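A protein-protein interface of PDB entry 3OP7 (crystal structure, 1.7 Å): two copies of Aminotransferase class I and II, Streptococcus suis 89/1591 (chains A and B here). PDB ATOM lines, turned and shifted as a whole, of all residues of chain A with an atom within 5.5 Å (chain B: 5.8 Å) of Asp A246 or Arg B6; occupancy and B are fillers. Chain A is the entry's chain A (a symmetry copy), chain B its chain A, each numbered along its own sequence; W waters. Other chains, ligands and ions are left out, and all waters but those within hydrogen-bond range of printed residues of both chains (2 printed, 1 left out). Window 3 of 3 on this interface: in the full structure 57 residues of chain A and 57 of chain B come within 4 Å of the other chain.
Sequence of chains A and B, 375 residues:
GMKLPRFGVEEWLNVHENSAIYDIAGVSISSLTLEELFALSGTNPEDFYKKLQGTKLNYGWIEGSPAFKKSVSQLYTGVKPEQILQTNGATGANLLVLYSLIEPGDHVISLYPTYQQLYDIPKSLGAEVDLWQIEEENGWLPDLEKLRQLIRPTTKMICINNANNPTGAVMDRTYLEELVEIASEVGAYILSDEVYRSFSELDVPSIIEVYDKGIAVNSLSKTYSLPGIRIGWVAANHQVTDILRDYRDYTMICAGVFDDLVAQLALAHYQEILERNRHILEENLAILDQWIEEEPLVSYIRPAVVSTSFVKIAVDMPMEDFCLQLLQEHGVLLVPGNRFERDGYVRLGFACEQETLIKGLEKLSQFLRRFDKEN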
ATOM      1  N   ASP A 242      34.977  10.826   5.252  1.00  0.00           N
ATOM      2  CA  ASP A 242      33.551  10.819   5.652  1.00  0.00           C
ATOM      3  C   ASP A 242      33.085  12.120   6.298  1.00  0.00           C
ATOM      4  O   ASP A 242      31.914  12.480   6.139  1.00  0.00           O
ATOM      5  CB  ASP A 242      33.249   9.703   6.643  1.00  0.00           C
ATOM      6  CG  ASP A 242      32.939   8.371   5.975  1.00  0.00           C
ATOM      7  OD1 ASP A 242      32.619   8.371   4.771  1.00  0.00           O
ATOM      8  OD2 ASP A 242      32.994   7.313   6.678  1.00  0.00           O
ATOM      9  N   ILE A 243      33.952  12.797   7.053  1.00  0.00           N
ATOM     10  CA  ILE A 243      33.587  14.100   7.617  1.00  0.00           C
ATOM     11  C   ILE A 243      33.425  15.135   6.516  1.00  0.00           C
ATOM     12  O   ILE A 243      32.368  15.796   6.387  1.00  0.00           O
ATOM     13  CB  ILE A 243      34.602  14.575   8.640  1.00  0.00           C
ATOM     14  CG1 ILE A 243      34.610  13.675   9.878  1.00  0.00           C
ATOM     15  CG2 ILE A 243      34.339  16.013   9.012  1.00  0.00           C
ATOM     16  CD1 ILE A 243      35.779  13.926  10.828  1.00  0.00           C
ATOM     17  N   LEU A 244      34.427  15.200   5.652  1.00  0.00           N
ATOM     18  CA  LEU A 244      34.466  16.249   4.607  1.00  0.00           C
ATOM     19  C   LEU A 244      33.254  16.203   3.692  1.00  0.00           C
ATOM     20  O   LEU A 244      32.822  17.221   3.211  1.00  0.00           O
ATOM     21  CB  LEU A 244      35.730  16.156   3.779  1.00  0.00           C
ATOM     22  CG  LEU A 244      37.071  16.226   4.506  1.00  0.00           C
ATOM     23  CD1 LEU A 244      38.305  16.281   3.536  1.00  0.00           C
ATOM     24  CD2 LEU A 244      37.191  17.344   5.510  1.00  0.00           C
ATOM     25  N   ARG A 245      32.732  15.005   3.432  1.00  0.00           N
ATOM     26  CA  ARG A 245      31.647  14.835   2.462  1.00  0.00           C
ATOM     27  C   ARG A 245      30.383  15.591   2.835  1.00  0.00           C
ATOM     28  O   ARG A 245      29.534  15.826   1.971  1.00  0.00           O
ATOM     29  CB  ARG A 245      31.239  13.380   2.345  1.00  0.00           C
ATOM     30  CG  ARG A 245      32.189  12.475   1.668  1.00  0.00           C
ATOM     31  CD  ARG A 245      31.435  11.190   1.412  1.00  0.00           C
ATOM     32  NE  ARG A 245      32.112  10.476   0.380  1.00  0.00           N
ATOM     33  CZ  ARG A 245      33.010   9.552   0.653  1.00  0.00           C
ATOM     34  NH1 ARG A 245      33.222   9.226   1.918  1.00  0.00           N
ATOM     35  NH2 ARG A 245      33.658   8.937  -0.323  1.00  0.00           N
ATOM     36  N   ASP A 246      30.249  15.924   4.107  1.00  0.00           N
ATOM     37  CA  ASP A 246      29.065  16.572   4.596  1.00  0.00           C
ATOM     38  C   ASP A 246      29.168  18.101   4.663  1.00  0.00           C
ATOM     39  O   ASP A 246      28.250  18.751   5.185  1.00  0.00           O
ATOM     40  CB  ASP A 246      28.698  16.017   5.964  1.00  0.00           C
ATOM     41  CG  ASP A 246      28.153  14.569   5.896  1.00  0.00           C
ATOM     42  OD1 ASP A 246      27.517  14.156   4.866  1.00  0.00           O
ATOM     43  OD2 ASP A 246      28.372  13.865   6.898  1.00  0.00           O
ATOM     44  N   TYR A 247      30.276  18.655   4.163  1.00  0.00           N
ATOM     45  CA  TYR A 247      30.518  20.108   4.191  1.00  0.00           C
ATOM     46  C   TYR A 247      30.734  20.742   2.815  1.00  0.00           C
ATOM     47  O   TYR A 247      30.828  21.969   2.701  1.00  0.00           O
ATOM     48  CB  TYR A 247      31.715  20.435   5.073  1.00  0.00           C
ATOM     49  CG  TYR A 247      31.474  20.081   6.503  1.00  0.00           C
ATOM     50  CD1 TYR A 247      30.865  20.992   7.374  1.00  0.00           C
ATOM     51  CD2 TYR A 247      31.797  18.823   6.976  1.00  0.00           C
ATOM     52  CE1 TYR A 247      30.608  20.641   8.682  1.00  0.00           C
ATOM     53  CE2 TYR A 247      31.558  18.465   8.264  1.00  0.00           C
ATOM     54  CZ  TYR A 247      30.960  19.371   9.121  1.00  0.00           C
ATOM     55  OH  TYR A 247      30.697  18.961  10.416  1.00  0.00           O
ATOM     56  N   ARG A 248      30.750  19.943   1.741  1.00  0.00           N
ATOM     57  CA  ARG A 248      31.023  20.505   0.424  1.00  0.00           C
ATOM     58  C   ARG A 248      29.923  21.466  -0.092  1.00  0.00           C
ATOM     59  O   ARG A 248      30.227  22.287  -0.920  1.00  0.00           O
ATOM     60  CB  ARG A 248      31.344  19.384  -0.588  1.00  0.00           C
ATOM     61  CG  ARG A 248      32.652  18.673  -0.169  1.00  0.00           C
ATOM     62  CD  ARG A 248      33.059  17.408  -0.997  1.00  0.00           C
ATOM     63  NE  ARG A 248      33.341  17.686  -2.401  1.00  0.00           N
ATOM     64  CZ  ARG A 248      32.541  17.412  -3.418  1.00  0.00           C
ATOM     65  NH1 ARG A 248      31.346  16.858  -3.220  1.00  0.00           N
ATOM     66  NH2 ARG A 248      32.913  17.723  -4.655  1.00  0.00           N
ATOM     67  N   ASP A 249      28.682  21.401   0.386  1.00  0.00           N
ATOM     68  CA  ASP A 249      27.700  22.390  -0.056  1.00  0.00           C
ATOM     69  C   ASP A 249      27.928  23.770   0.565  1.00  0.00           C
ATOM     70  O   ASP A 249      27.308  24.746   0.130  1.00  0.00           O
ATOM     71  CB  ASP A 249      26.246  21.983   0.154  1.00  0.00           C
ATOM     72  CG  ASP A 249      25.823  20.800  -0.702  1.00  0.00           C
ATOM     73  OD1 ASP A 249      26.691  20.202  -1.360  1.00  0.00           O
ATOM     74  OD2 ASP A 249      24.607  20.520  -0.668  1.00  0.00           O
ATOM     75  N   TYR A 250      28.820  23.896   1.531  1.00  0.00           N
ATOM     76  CA  TYR A 250      29.091  25.254   2.003  1.00  0.00           C
ATOM     77  C   TYR A 250      29.975  25.987   1.045  1.00  0.00           C
ATOM     78  O   TYR A 250      30.021  27.219   1.071  1.00  0.00           O
ATOM     79  CB  TYR A 250      29.806  25.207   3.363  1.00  0.00           C
ATOM     80  CG  TYR A 250      28.932  24.913   4.538  1.00  0.00           C
ATOM     81  CD1 TYR A 250      27.972  25.827   4.980  1.00  0.00           C
ATOM     82  CD2 TYR A 250      29.053  23.723   5.248  1.00  0.00           C
ATOM     83  CE1 TYR A 250      27.239  25.586   6.066  1.00  0.00           C
ATOM     84  CE2 TYR A 250      28.304  23.463   6.350  1.00  0.00           C
ATOM     85  CZ  TYR A 250      27.380  24.399   6.785  1.00  0.00           C
ATOM     86  OH  TYR A 250      26.519  24.213   7.875  1.00  0.00           O
ATOM     87  N   GLY B   1      30.299  19.933  12.830  1.00  0.00           N
ATOM     88  CA  GLY B   1      31.282  20.448  13.819  1.00  0.00           C
ATOM     89  C   GLY B   1      30.651  21.488  14.738  1.00  0.00           C
ATOM     90  O   GLY B   1      29.449  21.795  14.621  1.00  0.00           O
ATOM     91  N   LEU B   4      30.313  24.955  12.914  1.00  0.00           N
ATOM     92  CA  LEU B   4      29.862  24.699  11.522  1.00  0.00           C
ATOM     93  C   LEU B   4      29.253  23.302  11.464  1.00  0.00           C
ATOM     94  O   LEU B   4      29.993  22.327  11.385  1.00  0.00           O
ATOM     95  CB  LEU B   4      30.968  24.819  10.476  1.00  0.00           C
ATOM     96  CG  LEU B   4      30.452  24.802   9.036  1.00  0.00           C
ATOM     97  CD1 LEU B   4      29.708  26.102   8.664  1.00  0.00           C
ATOM     98  CD2 LEU B   4      31.603  24.539   8.021  1.00  0.00           C
ATOM     99  N   PRO B   5      27.910  23.219  11.550  1.00  0.00           N
ATOM    100  CA  PRO B   5      27.152  21.962  11.508  1.00  0.00           C
ATOM    101  C   PRO B   5      27.246  21.308  10.138  1.00  0.00           C
ATOM    102  O   PRO B   5      27.419  21.997   9.118  1.00  0.00           O
ATOM    103  CB  PRO B   5      25.673  22.408  11.787  1.00  0.00           C
ATOM    104  CG  PRO B   5      25.753  23.812  12.329  1.00  0.00           C
ATOM    105  CD  PRO B   5      27.032  24.389  11.681  1.00  0.00           C
ATOM    106  N   ARG B   6      27.139  19.991  10.080  1.00  0.00           N
ATOM    107  CA  ARG B   6      26.990  19.351   8.750  1.00  0.00           C
ATOM    108  C   ARG B   6      25.849  20.036   7.992  1.00  0.00           C
ATOM    109  O   ARG B   6      24.911  20.514   8.615  1.00  0.00           O
ATOM    110  CB  ARG B   6      26.641  17.880   8.922  1.00  0.00           C
ATOM    111  CG  ARG B   6      27.812  16.985   9.388  1.00  0.00           C
ATOM    112  CD  ARG B   6      27.282  15.594   9.785  1.00  0.00           C
ATOM    113  NE  ARG B   6      26.194  15.722  10.783  1.00  0.00           N
ATOM    114  CZ  ARG B   6      25.190  14.859  10.961  1.00  0.00           C
ATOM    115  NH1 ARG B   6      25.089  13.740  10.227  1.00  0.00           N
ATOM    116  NH2 ARG B   6      24.281  15.111  11.906  1.00  0.00           N
ATOM    117  N   PHE B   7      25.936  20.042   6.671  1.00  0.00           N
ATOM    118  CA  PHE B   7      24.955  20.656   5.789  1.00  0.00           C
ATOM    119  C   PHE B   7      23.822  19.620   5.633  1.00  0.00           C
ATOM    120  O   PHE B   7      24.032  18.541   5.101  1.00  0.00           O
ATOM    121  CB  PHE B   7      25.644  21.034   4.461  1.00  0.00           C
ATOM    122  CG  PHE B   7      24.952  22.132   3.687  1.00  0.00           C
ATOM    123  CD1 PHE B   7      23.692  21.902   3.100  1.00  0.00           C
ATOM    124  CD2 PHE B   7      25.568  23.370   3.491  1.00  0.00           C
ATOM    125  CE1 PHE B   7      23.061  22.883   2.363  1.00  0.00           C
ATOM    126  CE2 PHE B   7      24.960  24.368   2.769  1.00  0.00           C
ATOM    127  CZ  PHE B   7      23.695  24.124   2.170  1.00  0.00           C
ATOM    128  N   GLY B   8      22.642  19.937   6.183  1.00  0.00           N
ATOM    129  CA  GLY B   8      21.617  18.949   6.400  1.00  0.00           C
ATOM    130  C   GLY B   8      21.055  18.306   5.155  1.00  0.00           C
ATOM    131  O   GLY B   8      20.917  17.084   5.109  1.00  0.00           O
ATOM    132  N   GLU B  10      22.490  18.152   2.274  1.00  0.00           N
ATOM    133  CA  GLU B  10      23.630  17.404   1.717  1.00  0.00           C
ATOM    134  C   GLU B  10      23.832  15.999   2.325  1.00  0.00           C
ATOM    135  O   GLU B  10      24.009  14.986   1.617  1.00  0.00           O
ATOM    136  CB  GLU B  10      24.942  18.245   1.871  1.00  0.00           C
ATOM    137  CG  GLU B  10      26.139  17.598   1.236  1.00  0.00           C
ATOM    138  CD  GLU B  10      27.431  18.475   1.345  1.00  0.00           C
ATOM    139  OE1 GLU B  10      27.381  19.514   2.000  1.00  0.00           O
ATOM    140  OE2 GLU B  10      28.457  18.061   0.759  1.00  0.00           O
ATOM    141  N   GLU B  11      23.797  15.917   3.652  1.00  0.00           N
ATOM    142  CA  GLU B  11      24.009  14.663   4.338  1.00  0.00           C
ATOM    143  C   GLU B  11      22.884  13.681   3.920  1.00  0.00           C
ATOM    144  O   GLU B  11      23.131  12.509   3.635  1.00  0.00           O
ATOM    145  CB  GLU B  11      23.998  14.902   5.858  1.00  0.00           C
ATOM    146  CG  GLU B  11      24.438  13.672   6.701  1.00  0.00           C
ATOM    147  CD  GLU B  11      23.306  12.669   6.987  1.00  0.00           C
ATOM    148  OE1 GLU B  11      22.115  13.077   6.961  1.00  0.00           O
ATOM    149  OE2 GLU B  11      23.603  11.457   7.223  1.00  0.00           O
ATOM    150  N   ASN B  14      23.605  12.706   0.279  1.00  0.00           N
ATOM    151  CA  ASN B  14      24.761  11.803   0.247  1.00  0.00           C
ATOM    152  C   ASN B  14      24.373  10.354   0.559  1.00  0.00           C
ATOM    153  O   ASN B  14      24.810   9.412  -0.120  1.00  0.00           O
ATOM    154  CB  ASN B  14      25.838  12.224   1.257  1.00  0.00           C
ATOM    155  CG  ASN B  14      26.630  13.432   0.823  1.00  0.00           C
ATOM    156  OD1 ASN B  14      26.632  13.827  -0.348  1.00  0.00           O
ATOM    157  ND2 ASN B  14      27.310  14.045   1.781  1.00  0.00           N
ATOM    158  N   GLN B 116      20.999  26.851   3.889  1.00  0.00           N
ATOM    159  CA  GLN B 116      21.783  26.761   5.136  1.00  0.00           C
ATOM    160  C   GLN B 116      23.040  27.631   5.180  1.00  0.00           C
ATOM    161  O   GLN B 116      23.470  28.044   6.240  1.00  0.00           O
ATOM    162  CB  GLN B 116      22.117  25.284   5.463  1.00  0.00           C
ATOM    163  CG  GLN B 116      22.821  25.068   6.795  1.00  0.00           C
ATOM    164  CD  GLN B 116      23.001  23.604   7.157  1.00  0.00           C
ATOM    165  OE1 GLN B 116      22.445  22.719   6.493  1.00  0.00           O
ATOM    166  NE2 GLN B 116      23.755  23.341   8.225  1.00  0.00           N
ATOM    167  N   ASP B 120      24.469  29.521   8.786  1.00  0.00           N
ATOM    168  CA  ASP B 120      25.569  28.784   9.394  1.00  0.00           C
ATOM    169  C   ASP B 120      26.945  29.304   9.036  1.00  0.00           C
ATOM    170  O   ASP B 120      27.851  29.226   9.865  1.00  0.00           O
ATOM    171  CB  ASP B 120      25.412  27.278   9.190  1.00  0.00           C
ATOM    172  CG  ASP B 120      24.495  26.639  10.245  1.00  0.00           C
ATOM    173  OD1 ASP B 120      24.324  27.239  11.367  1.00  0.00           O
ATOM    174  OD2 ASP B 120      23.939  25.536   9.955  1.00  0.00           O
HETATM  175  O   HOH W   1      27.090  12.340   8.646  1.00  0.00           O
HETATM  176  O   HOH W   2      32.638  21.417  11.023  1.00  0.00           O
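The backbone NH of Gly B1 is in hydrogen-bond range of the side-chain hydroxyl of Tyr A247 (2.6 Å).
O of Pro B5 is in hydrogen-bond range of OH of Tyr A250, 2.7 Å away.
N of Phe B7 lies within hydrogen-bond range of O of Asp A246 (3.0 Å).
N of Arg A248 lies within hydrogen-bond range of OE2 of Glu B10 (3.1 Å).
The side-chain carboxylate of Glu B10 is in hydrogen-bond range of the backbone NH of Asp A249 (2.8 Å).
The side-chain amide nitrogen (ND2) of Asn B14 is in hydrogen-bond range of the backbone carbonyl oxygen (O) of Arg A245, at 2.9 Å.
ND2 of Asn B14 is in hydrogen-bond range of OD1 of Asp A246, 3.1 Å away.
The side-chain hydroxyl (OH) of Tyr A250 sits at hydrogen-bond distance from the side-chain amide nitrogen (NE2) of Gln B116 (2.9 Å).
O of Arg A245 lies close to OE2 of Glu B10, at 2.8 Å.
The backbone carbonyl oxygen (O) of Asp A246 sits close to the side-chain carboxylate (OE1) of Glu B10 (3.4 Å).
The backbone carbonyl oxygen (O) of Arg B6 sits at hydrogen-bond distance from the side-chain amide nitrogen (NE2) of Gln B116 (3.1 Å).
The backbone NH (N) of Gly B8 sits at hydrogen-bond distance from the side-chain amide oxygen (OE1) of Gln B116, at 2.8 Å.
The backbone carbonyl oxygen (O) of Glu B10 sits close to the side-chain amide nitrogen (ND2) of Asn B14 (3.4 Å).
NE2 of Gln B116 lies within hydrogen-bond range of OD2 of Asp B120 (2.8 Å).
OD1 of Asp A242 is in salt-bridge range of NH1 of Arg A245.
Arg B6 touches Asp A246 (CD to OD2, 3.5 Å).
Glu B11 touches Asp A246 (CA to OD1, 3.6 Å).
CE1 of Tyr A247 touches O of Leu B4, 3.2 Å away.
Pro B5 touches Tyr A247 (O to CE1, 3.5 Å).
CG of Arg B6 touches OH of Tyr A247, 3.6 Å away.
Tyr A247 touches Glu B10.
Asp A249 touches Phe B7.
Leu B4 touches Tyr A250.
Phe B7 touches Tyr A250.
Asp B120 touches Tyr A250 (CB to OH, 3.5 Å).
Asp A246 touches just these residues of chain B: Arg B6 (3.5 Å), Phe B7 (3.0 Å), Glu B10 (3.4 Å), Glu B11 (3.6 Å) and Asn B14 (3.1 Å).
Arg B6 touches just these residues of chain A: Asp A246 (3.5 Å) and Tyr A247 (3.6 Å).
Printed residues of chain A within 4 Å of Pro B5: Tyr A247 (3.5 Å) and Tyr A250 (2.7 Å).
Printed residues of chain B within 4 Å of Tyr A250: Leu B4 (3.4 Å), Pro B5 (2.7 Å), Phe B7 (3.7 Å), Gln B116 (2.9 Å) and Asp B120 (3.5 Å).
Printed residues of chain B within 4 Å of Tyr A247: Gly B1, Leu B4, Pro B5, Arg B6 and Glu B10.
The nearest residue of chain B that does not touch Asp A246 is Pro B5 (5.2 Å).
The nearest printed residue of chain B that does not touch Tyr A247 is Phe B7 (5.0 Å).
Printed residues of chain A that touch a printed residue of chain B: Arg A245, Asp A246, Tyr A247, Arg A248, Asp A249 and Tyr A250.
Hydrophobic or aromatic side chains of chain A that line the printed part of chain B: Tyr A247 and Tyr A250.
Of the 11 printed residues of chain B, 10 touch a printed residue of chain A.
Printed residues of chain B that touch a printed residue of chain A: Gly B1, Leu B4, Pro B5, Arg B6, Phe B7, Glu B10, Glu B11, Asn B14, Gln B116 and Asp B120.
Along chain B the printed residues that touch a printed residue of chain A span positions 1 to 120.
Among the printed residues, 20 pairs touch across the chains.
Among the printed residues, no Asp or Glu carboxylate lies within 4 Å of a Lys or Arg side-chain nitrogen of the other chain.
No position is printed for both chains.
Water W1 bridges the side-chain carboxylate (OD2) of Asp A246 (2.7 Å) and the guanidinium group (NH1) of Arg B6 (2.9 Å).
Water W2 lies within hydrogen-bond range of the backbone carbonyl oxygen (O) of Leu B4 (2.8 Å), the side-chain hydroxyl (OH) of Tyr A247 (3.2 Å) and the backbone NH (N) of Gly B1 (3.3 Å).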
